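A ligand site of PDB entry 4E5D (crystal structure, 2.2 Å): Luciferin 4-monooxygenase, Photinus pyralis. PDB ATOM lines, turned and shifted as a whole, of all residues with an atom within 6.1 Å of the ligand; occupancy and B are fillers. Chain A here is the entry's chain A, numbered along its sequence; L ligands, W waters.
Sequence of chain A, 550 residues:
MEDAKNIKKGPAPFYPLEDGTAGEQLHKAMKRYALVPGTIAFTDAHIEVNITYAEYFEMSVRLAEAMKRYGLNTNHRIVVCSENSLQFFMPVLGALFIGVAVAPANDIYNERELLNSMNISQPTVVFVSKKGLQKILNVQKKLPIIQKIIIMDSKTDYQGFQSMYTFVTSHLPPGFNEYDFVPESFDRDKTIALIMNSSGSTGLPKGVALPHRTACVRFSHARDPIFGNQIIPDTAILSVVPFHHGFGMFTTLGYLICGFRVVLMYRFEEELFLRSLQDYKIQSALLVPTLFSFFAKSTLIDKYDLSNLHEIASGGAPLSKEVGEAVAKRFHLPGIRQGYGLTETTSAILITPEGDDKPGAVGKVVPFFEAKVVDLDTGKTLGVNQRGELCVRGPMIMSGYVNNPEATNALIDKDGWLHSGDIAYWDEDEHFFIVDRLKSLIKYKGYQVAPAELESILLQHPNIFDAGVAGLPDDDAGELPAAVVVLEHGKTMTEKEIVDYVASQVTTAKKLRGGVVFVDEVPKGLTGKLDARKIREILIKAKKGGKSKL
The backbone NH (N) of Leu 342 is in hydrogen-bond range of the side-chain hydroxyl (OG1) of Thr 345 (3.0 Å).
The backbone carbonyl oxygen (O) of Phe 247 sits at hydrogen-bond distance from the side-chain hydroxyl (OG1) of Thr 251 (2.7 Å).
The side-chain hydroxyl (OG1) of Thr 345 is in hydrogen-bond range of the backbone carbonyl oxygen (O) of Ser 347 (2.9 Å).
O of Arg 337 lies within hydrogen-bond range of N of Ser 314, 2.9 Å away.
A ring nitrogen (ND1) of His 245 lies within hydrogen-bond range of the backbone NH (N) of Phe 247, at 3.1 Å.
O of Ser 314 sits at hydrogen-bond distance from N of Gly 339 (3.0 Å).
Water W1 lies within hydrogen-bond range of the side-chain hydroxyl (OG) of Ser 347 (2.5 Å), a nitrogen (N1) of the ligand (2.6 Å) and the backbone carbonyl oxygen (O) of Gly 246 (3.1 Å).
A nitrogen (N1) of the ligand sits at hydrogen-bond distance from the backbone NH of Ala 348.
The side-chain hydroxyl (OG) of Ser 347 sits close to a nitrogen (N1) of the ligand (3.5 Å).
CE1 of His 245 touches C2 of the ligand (3.6 Å).
Gly 246 touches the ligand (C to C4, 3.7 Å).
Phe 247 touches the ligand.
Thr 251 touches the ligand (CG2 to C10, 3.7 Å).
CB of Ala 313 touches C14 of the ligand (3.6 Å).
Ser 314 touches the ligand (O to C13, 3.7 Å).
CA of Gly 315 touches S1 of the ligand (3.2 Å).
Arg 337 touches the ligand.
Gln 338 touches the ligand.
Gly 339 touches the ligand (CA to C13, 3.5 Å).
Gly 341 touches the ligand.
Leu 342 touches the ligand.
Thr 343 touches the ligand.
Thr 346 touches the ligand (O to C4, 3.5 Å).
Of the 24 residues printed, 16 come within 4 Å of the ligand.
The nearest printed residue that does not touch the ligand is Arg 218 (4.1 Å).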
ATOM      1  N   ARG A 218      20.929 -22.509 -27.278  1.00  0.00           N
ATOM      2  CA  ARG A 218      19.992 -21.923 -28.210  1.00  0.00           C
ATOM      3  C   ARG A 218      19.951 -22.759 -29.491  1.00  0.00           C
ATOM      4  O   ARG A 218      18.871 -22.994 -30.055  1.00  0.00           O
ATOM      5  CB  ARG A 218      20.337 -20.447 -28.471  1.00  0.00           C
ATOM      6  CG  ARG A 218      19.524 -19.832 -29.603  1.00  0.00           C
ATOM      7  CD  ARG A 218      18.023 -19.806 -29.323  1.00  0.00           C
ATOM      8  NE  ARG A 218      17.250 -19.551 -30.555  1.00  0.00           N
ATOM      9  CZ  ARG A 218      15.960 -19.824 -30.703  1.00  0.00           C
ATOM     10  NH1 ARG A 218      15.258 -20.317 -29.673  1.00  0.00           N
ATOM     11  NH2 ARG A 218      15.354 -19.598 -31.863  1.00  0.00           N
ATOM     12  N   PHE A 227      10.276 -27.143 -29.796  1.00  0.00           N
ATOM     13  CA  PHE A 227      10.573 -25.833 -29.218  1.00  0.00           C
ATOM     14  C   PHE A 227      11.219 -24.884 -30.219  1.00  0.00           C
ATOM     15  O   PHE A 227      11.506 -23.718 -29.892  1.00  0.00           O
ATOM     16  CB  PHE A 227      11.433 -25.991 -27.970  1.00  0.00           C
ATOM     17  CG  PHE A 227      10.688 -26.620 -26.835  1.00  0.00           C
ATOM     18  CD1 PHE A 227       9.852 -25.857 -26.028  1.00  0.00           C
ATOM     19  CD2 PHE A 227      10.762 -27.968 -26.606  1.00  0.00           C
ATOM     20  CE1 PHE A 227       9.132 -26.442 -24.988  1.00  0.00           C
ATOM     21  CE2 PHE A 227      10.059 -28.546 -25.588  1.00  0.00           C
ATOM     22  CZ  PHE A 227       9.234 -27.775 -24.779  1.00  0.00           C
ATOM     23  N   HIS A 245      19.567  -6.929 -31.396  1.00  0.00           N
ATOM     24  CA  HIS A 245      18.797  -7.245 -30.212  1.00  0.00           C
ATOM     25  C   HIS A 245      18.716  -8.771 -30.126  1.00  0.00           C
ATOM     26  O   HIS A 245      18.793  -9.463 -31.139  1.00  0.00           O
ATOM     27  CB  HIS A 245      17.409  -6.557 -30.313  1.00  0.00           C
ATOM     28  CG  HIS A 245      16.484  -6.859 -29.177  1.00  0.00           C
ATOM     29  ND1 HIS A 245      15.736  -8.020 -29.128  1.00  0.00           N
ATOM     30  CD2 HIS A 245      16.164  -6.154 -28.060  1.00  0.00           C
ATOM     31  CE1 HIS A 245      14.991  -8.023 -28.030  1.00  0.00           C
ATOM     32  NE2 HIS A 245      15.235  -6.906 -27.365  1.00  0.00           N
ATOM     33  N   GLY A 246      18.599  -9.298 -28.910  1.00  0.00           N
ATOM     34  CA  GLY A 246      18.652 -10.729 -28.689  1.00  0.00           C
ATOM     35  C   GLY A 246      17.641 -11.522 -29.490  1.00  0.00           C
ATOM     36  O   GLY A 246      17.929 -12.608 -29.959  1.00  0.00           O
ATOM     37  N   PHE A 247      16.420 -10.998 -29.592  1.00  0.00           N
ATOM     38  CA  PHE A 247      15.391 -11.609 -30.428  1.00  0.00           C
ATOM     39  C   PHE A 247      15.880 -11.820 -31.867  1.00  0.00           C
ATOM     40  O   PHE A 247      15.725 -12.895 -32.431  1.00  0.00           O
ATOM     41  CB  PHE A 247      14.085 -10.765 -30.376  1.00  0.00           C
ATOM     42  CG  PHE A 247      12.894 -11.432 -31.032  1.00  0.00           C
ATOM     43  CD1 PHE A 247      12.901 -12.793 -31.330  1.00  0.00           C
ATOM     44  CD2 PHE A 247      11.762 -10.690 -31.352  1.00  0.00           C
ATOM     45  CE1 PHE A 247      11.793 -13.398 -31.920  1.00  0.00           C
ATOM     46  CE2 PHE A 247      10.638 -11.301 -31.966  1.00  0.00           C
ATOM     47  CZ  PHE A 247      10.660 -12.651 -32.248  1.00  0.00           C
ATOM     48  N   PHE A 250      19.555 -14.143 -31.870  1.00  0.00           N
ATOM     49  CA  PHE A 250      19.539 -15.550 -31.509  1.00  0.00           C
ATOM     50  C   PHE A 250      18.556 -16.374 -32.308  1.00  0.00           C
ATOM     51  O   PHE A 250      18.756 -17.588 -32.464  1.00  0.00           O
ATOM     52  CB  PHE A 250      19.429 -15.707 -29.988  1.00  0.00           C
ATOM     53  CG  PHE A 250      20.698 -15.280 -29.280  1.00  0.00           C
ATOM     54  CD1 PHE A 250      21.876 -16.026 -29.442  1.00  0.00           C
ATOM     55  CD2 PHE A 250      20.744 -14.100 -28.560  1.00  0.00           C
ATOM     56  CE1 PHE A 250      23.056 -15.615 -28.843  1.00  0.00           C
ATOM     57  CE2 PHE A 250      21.904 -13.700 -27.953  1.00  0.00           C
ATOM     58  CZ  PHE A 250      23.075 -14.436 -28.108  1.00  0.00           C
ATOM     59  N   THR A 251      17.559 -15.730 -32.899  1.00  0.00           N
ATOM     60  CA  THR A 251      16.755 -16.433 -33.880  1.00  0.00           C
ATOM     61  C   THR A 251      17.591 -16.651 -35.148  1.00  0.00           C
ATOM     62  O   THR A 251      17.598 -17.735 -35.720  1.00  0.00           O
ATOM     63  CB  THR A 251      15.427 -15.664 -34.211  1.00  0.00           C
ATOM     64  OG1 THR A 251      15.730 -14.353 -34.670  1.00  0.00           O
ATOM     65  CG2 THR A 251      14.469 -15.581 -32.962  1.00  0.00           C
ATOM     66  N   ALA A 313       5.740 -15.640 -35.266  1.00  0.00           N
ATOM     67  CA  ALA A 313       6.422 -15.706 -33.984  1.00  0.00           C
ATOM     68  C   ALA A 313       6.503 -14.349 -33.289  1.00  0.00           C
ATOM     69  O   ALA A 313       6.838 -13.337 -33.917  1.00  0.00           O
ATOM     70  CB  ALA A 313       7.808 -16.273 -34.185  1.00  0.00           C
ATOM     71  N   SER A 314       6.228 -14.327 -31.999  1.00  0.00           N
ATOM     72  CA  SER A 314       6.256 -13.106 -31.196  1.00  0.00           C
ATOM     73  C   SER A 314       7.308 -13.184 -30.097  1.00  0.00           C
ATOM     74  O   SER A 314       7.344 -14.142 -29.315  1.00  0.00           O
ATOM     75  CB  SER A 314       4.911 -12.895 -30.495  1.00  0.00           C
ATOM     76  OG  SER A 314       4.835 -11.601 -29.923  1.00  0.00           O
ATOM     77  N   GLY A 315       8.135 -12.146 -30.008  1.00  0.00           N
ATOM     78  CA  GLY A 315       9.162 -12.051 -28.970  1.00  0.00           C
ATOM     79  C   GLY A 315       8.615 -11.940 -27.554  1.00  0.00           C
ATOM     80  O   GLY A 315       8.096 -10.908 -27.123  1.00  0.00           O
ATOM     81  N   ARG A 337       2.747 -18.110 -32.333  1.00  0.00           N
ATOM     82  CA  ARG A 337       3.880 -18.814 -31.751  1.00  0.00           C
ATOM     83  C   ARG A 337       4.607 -17.827 -30.844  1.00  0.00           C
ATOM     84  O   ARG A 337       5.453 -17.082 -31.310  1.00  0.00           O
ATOM     85  CB  ARG A 337       4.813 -19.319 -32.858  1.00  0.00           C
ATOM     86  CG  ARG A 337       5.935 -20.169 -32.343  1.00  0.00           C
ATOM     87  CD  ARG A 337       5.517 -21.584 -32.394  1.00  0.00           C
ATOM     88  NE  ARG A 337       6.448 -22.499 -31.733  1.00  0.00           N
ATOM     89  CZ  ARG A 337       7.422 -23.181 -32.334  1.00  0.00           C
ATOM     90  NH1 ARG A 337       7.650 -23.045 -33.644  1.00  0.00           N
ATOM     91  NH2 ARG A 337       8.145 -24.029 -31.625  1.00  0.00           N
ATOM     92  N   GLN A 338       4.236 -17.798 -29.570  1.00  0.00           N
ATOM     93  CA  GLN A 338       4.821 -16.871 -28.616  1.00  0.00           C
ATOM     94  C   GLN A 338       6.032 -17.446 -27.941  1.00  0.00           C
ATOM     95  O   GLN A 338       6.173 -18.661 -27.801  1.00  0.00           O
ATOM     96  CB  GLN A 338       3.821 -16.480 -27.526  1.00  0.00           C
ATOM     97  CG  GLN A 338       2.598 -15.807 -28.030  1.00  0.00           C
ATOM     98  CD  GLN A 338       1.678 -15.326 -26.903  1.00  0.00           C
ATOM     99  OE1 GLN A 338       2.085 -14.531 -26.038  1.00  0.00           O
ATOM    100  NE2 GLN A 338       0.435 -15.772 -26.935  1.00  0.00           N
ATOM    101  N   GLY A 339       6.907 -16.524 -27.532  1.00  0.00           N
ATOM    102  CA  GLY A 339       8.099 -16.841 -26.793  1.00  0.00           C
ATOM    103  C   GLY A 339       8.288 -15.766 -25.751  1.00  0.00           C
ATOM    104  O   GLY A 339       7.853 -14.629 -25.921  1.00  0.00           O
ATOM    105  N   TYR A 340       8.919 -16.121 -24.642  1.00  0.00           N
ATOM    106  CA  TYR A 340       9.239 -15.138 -23.614  1.00  0.00           C
ATOM    107  C   TYR A 340      10.704 -15.315 -23.246  1.00  0.00           C
ATOM    108  O   TYR A 340      11.147 -16.418 -22.966  1.00  0.00           O
ATOM    109  CB  TYR A 340       8.373 -15.340 -22.363  1.00  0.00           C
ATOM    110  CG  TYR A 340       8.788 -14.441 -21.236  1.00  0.00           C
ATOM    111  CD1 TYR A 340       8.298 -13.148 -21.127  1.00  0.00           C
ATOM    112  CD2 TYR A 340       9.717 -14.864 -20.282  1.00  0.00           C
ATOM    113  CE1 TYR A 340       8.687 -12.312 -20.087  1.00  0.00           C
ATOM    114  CE2 TYR A 340      10.129 -14.014 -19.238  1.00  0.00           C
ATOM    115  CZ  TYR A 340       9.592 -12.751 -19.138  1.00  0.00           C
ATOM    116  OH  TYR A 340       9.988 -11.907 -18.118  1.00  0.00           O
ATOM    117  N   GLY A 341      11.446 -14.226 -23.241  1.00  0.00           N
ATOM    118  CA  GLY A 341      12.836 -14.250 -22.869  1.00  0.00           C
ATOM    119  C   GLY A 341      13.287 -12.842 -22.574  1.00  0.00           C
ATOM    120  O   GLY A 341      12.568 -11.892 -22.813  1.00  0.00           O
ATOM    121  N   LEU A 342      14.494 -12.730 -22.029  1.00  0.00           N
ATOM    122  CA  LEU A 342      15.116 -11.436 -21.789  1.00  0.00           C
ATOM    123  C   LEU A 342      16.525 -11.488 -22.380  1.00  0.00           C
ATOM    124  O   LEU A 342      17.076 -12.553 -22.649  1.00  0.00           O
ATOM    125  CB  LEU A 342      15.228 -11.155 -20.282  1.00  0.00           C
ATOM    126  CG  LEU A 342      13.926 -11.256 -19.505  1.00  0.00           C
ATOM    127  CD1 LEU A 342      14.256 -11.305 -18.054  1.00  0.00           C
ATOM    128  CD2 LEU A 342      13.002 -10.093 -19.846  1.00  0.00           C
ATOM    129  N   THR A 343      17.118 -10.322 -22.528  1.00  0.00           N
ATOM    130  CA  THR A 343      18.476 -10.243 -22.993  1.00  0.00           C
ATOM    131  C   THR A 343      19.348 -11.092 -22.033  1.00  0.00           C
ATOM    132  O   THR A 343      20.189 -11.878 -22.484  1.00  0.00           O
ATOM    133  CB  THR A 343      18.928  -8.782 -23.048  1.00  0.00           C
ATOM    134  OG1 THR A 343      17.983  -8.035 -23.822  1.00  0.00           O
ATOM    135  CG2 THR A 343      20.312  -8.678 -23.688  1.00  0.00           C
ATOM    136  N   GLU A 344      19.063 -10.979 -20.738  1.00  0.00           N
ATOM    137  CA  GLU A 344      19.785 -11.677 -19.694  1.00  0.00           C
ATOM    138  C   GLU A 344      19.587 -13.171 -19.732  1.00  0.00           C
ATOM    139  O   GLU A 344      20.319 -13.879 -19.053  1.00  0.00           O
ATOM    140  CB  GLU A 344      19.391 -11.165 -18.302  1.00  0.00           C
ATOM    141  CG  GLU A 344      19.776  -9.722 -18.046  1.00  0.00           C
ATOM    142  CD  GLU A 344      18.836  -8.684 -18.672  1.00  0.00           C
ATOM    143  OE1 GLU A 344      17.921  -9.043 -19.446  1.00  0.00           O
ATOM    144  OE2 GLU A 344      19.015  -7.487 -18.380  1.00  0.00           O
ATOM    145  N   THR A 345      18.614 -13.658 -20.521  1.00  0.00           N
ATOM    146  CA  THR A 345      18.444 -15.118 -20.683  1.00  0.00           C
ATOM    147  C   THR A 345      18.828 -15.629 -22.073  1.00  0.00           C
ATOM    148  O   THR A 345      18.421 -16.739 -22.455  1.00  0.00           O
ATOM    149  CB  THR A 345      16.979 -15.596 -20.351  1.00  0.00           C
ATOM    150  OG1 THR A 345      16.062 -15.191 -21.385  1.00  0.00           O
ATOM    151  CG2 THR A 345      16.555 -15.044 -19.024  1.00  0.00           C
ATOM    152  N   THR A 346      19.581 -14.807 -22.805  1.00  0.00           N
ATOM    153  CA  THR A 346      20.035 -15.087 -24.183  1.00  0.00           C
ATOM    154  C   THR A 346      18.898 -15.067 -25.220  1.00  0.00           C
ATOM    155  O   THR A 346      18.870 -14.181 -26.112  1.00  0.00           O
ATOM    156  CB  THR A 346      20.763 -16.426 -24.309  1.00  0.00           C
ATOM    157  OG1 THR A 346      21.940 -16.404 -23.486  1.00  0.00           O
ATOM    158  CG2 THR A 346      21.189 -16.675 -25.782  1.00  0.00           C
ATOM    159  N   SER A 347      18.009 -16.046 -25.106  1.00  0.00           N
ATOM    160  CA  SER A 347      16.851 -16.174 -25.979  1.00  0.00           C
ATOM    161  C   SER A 347      15.571 -16.575 -25.185  1.00  0.00           C
ATOM    162  O   SER A 347      15.521 -16.434 -23.960  1.00  0.00           O
ATOM    163  CB  SER A 347      17.151 -17.228 -27.054  1.00  0.00           C
ATOM    164  OG  SER A 347      16.159 -17.161 -28.066  1.00  0.00           O
ATOM    165  N   ALA A 348      14.547 -17.085 -25.863  1.00  0.00           N
ATOM    166  CA  ALA A 348      13.324 -17.456 -25.154  1.00  0.00           C
ATOM    167  C   ALA A 348      13.565 -18.672 -24.293  1.00  0.00           C
ATOM    168  O   ALA A 348      14.123 -19.677 -24.750  1.00  0.00           O
ATOM    169  CB  ALA A 348      12.193 -17.716 -26.115  1.00  0.00           C
ATOM    170  N   LEU A 350      10.683 -19.546 -22.267  1.00  0.00           N
ATOM    171  CA  LEU A 350       9.346 -20.111 -22.429  1.00  0.00           C
ATOM    172  C   LEU A 350       8.950 -19.982 -23.895  1.00  0.00           C
ATOM    173  O   LEU A 350       9.071 -18.913 -24.492  1.00  0.00           O
ATOM    174  CB  LEU A 350       8.318 -19.381 -21.540  1.00  0.00           C
ATOM    175  CG  LEU A 350       8.633 -19.460 -20.045  1.00  0.00           C
ATOM    176  CD1 LEU A 350       7.756 -18.503 -19.286  1.00  0.00           C
ATOM    177  CD2 LEU A 350       8.430 -20.914 -19.576  1.00  0.00           C
ATOM    178  N   ILE A 351       8.470 -21.077 -24.475  1.00  0.00           N
ATOM    179  CA  ILE A 351       8.132 -21.109 -25.877  1.00  0.00           C
ATOM    180  C   ILE A 351       6.919 -22.002 -26.147  1.00  0.00           C
ATOM    181  O   ILE A 351       6.865 -23.117 -25.644  1.00  0.00           O
ATOM    182  CB  ILE A 351       9.319 -21.642 -26.707  1.00  0.00           C
ATOM    183  CG1 ILE A 351      10.520 -20.692 -26.565  1.00  0.00           C
ATOM    184  CG2 ILE A 351       8.922 -21.801 -28.170  1.00  0.00           C
ATOM    185  CD1 ILE A 351      11.831 -21.237 -27.203  1.00  0.00           C
HETATM  186  F1  LIG L   1      12.170 -11.354 -26.289  1.00  0.00           F
HETATM  187  C1  LIG L   1      13.498 -11.508 -26.219  1.00  0.00           C
HETATM  188  C2  LIG L   1      14.299 -10.544 -25.614  1.00  0.00           C
HETATM  189  C3  LIG L   1      15.672 -10.708 -25.569  1.00  0.00           C
HETATM  190  C4  LIG L   1      16.236 -11.851 -26.114  1.00  0.00           C
HETATM  191  C5  LIG L   1      15.438 -12.825 -26.702  1.00  0.00           C
HETATM  192  C6  LIG L   1      14.065 -12.662 -26.747  1.00  0.00           C
HETATM  193  C7  LIG L   1      13.228 -13.674 -27.443  1.00  0.00           C
HETATM  194  S1  LIG L   1      11.518 -13.787 -27.562  1.00  0.00           S
HETATM  195  C8  LIG L   1      11.510 -15.193 -28.596  1.00  0.00           C
HETATM  196  N1  LIG L   1      13.760 -14.637 -28.218  1.00  0.00           N
HETATM  197  C9  LIG L   1      12.853 -15.511 -28.838  1.00  0.00           C
HETATM  198  C10 LIG L   1      13.226 -16.608 -29.661  1.00  0.00           C
HETATM  199  C11 LIG L   1      12.250 -17.398 -30.258  1.00  0.00           C
HETATM  200  C12 LIG L   1      10.900 -17.101 -30.038  1.00  0.00           C
HETATM  201  C13 LIG L   1      10.536 -16.001 -29.226  1.00  0.00           C
HETATM  202  O1  LIG L   1       9.936 -17.898 -30.629  1.00  0.00           O
HETATM  203  C14 LIG L   1       8.654 -17.419 -30.839  1.00  0.00           C
HETATM  204  O   HOH W   1      16.120 -14.991 -29.290  1.00  0.00           O
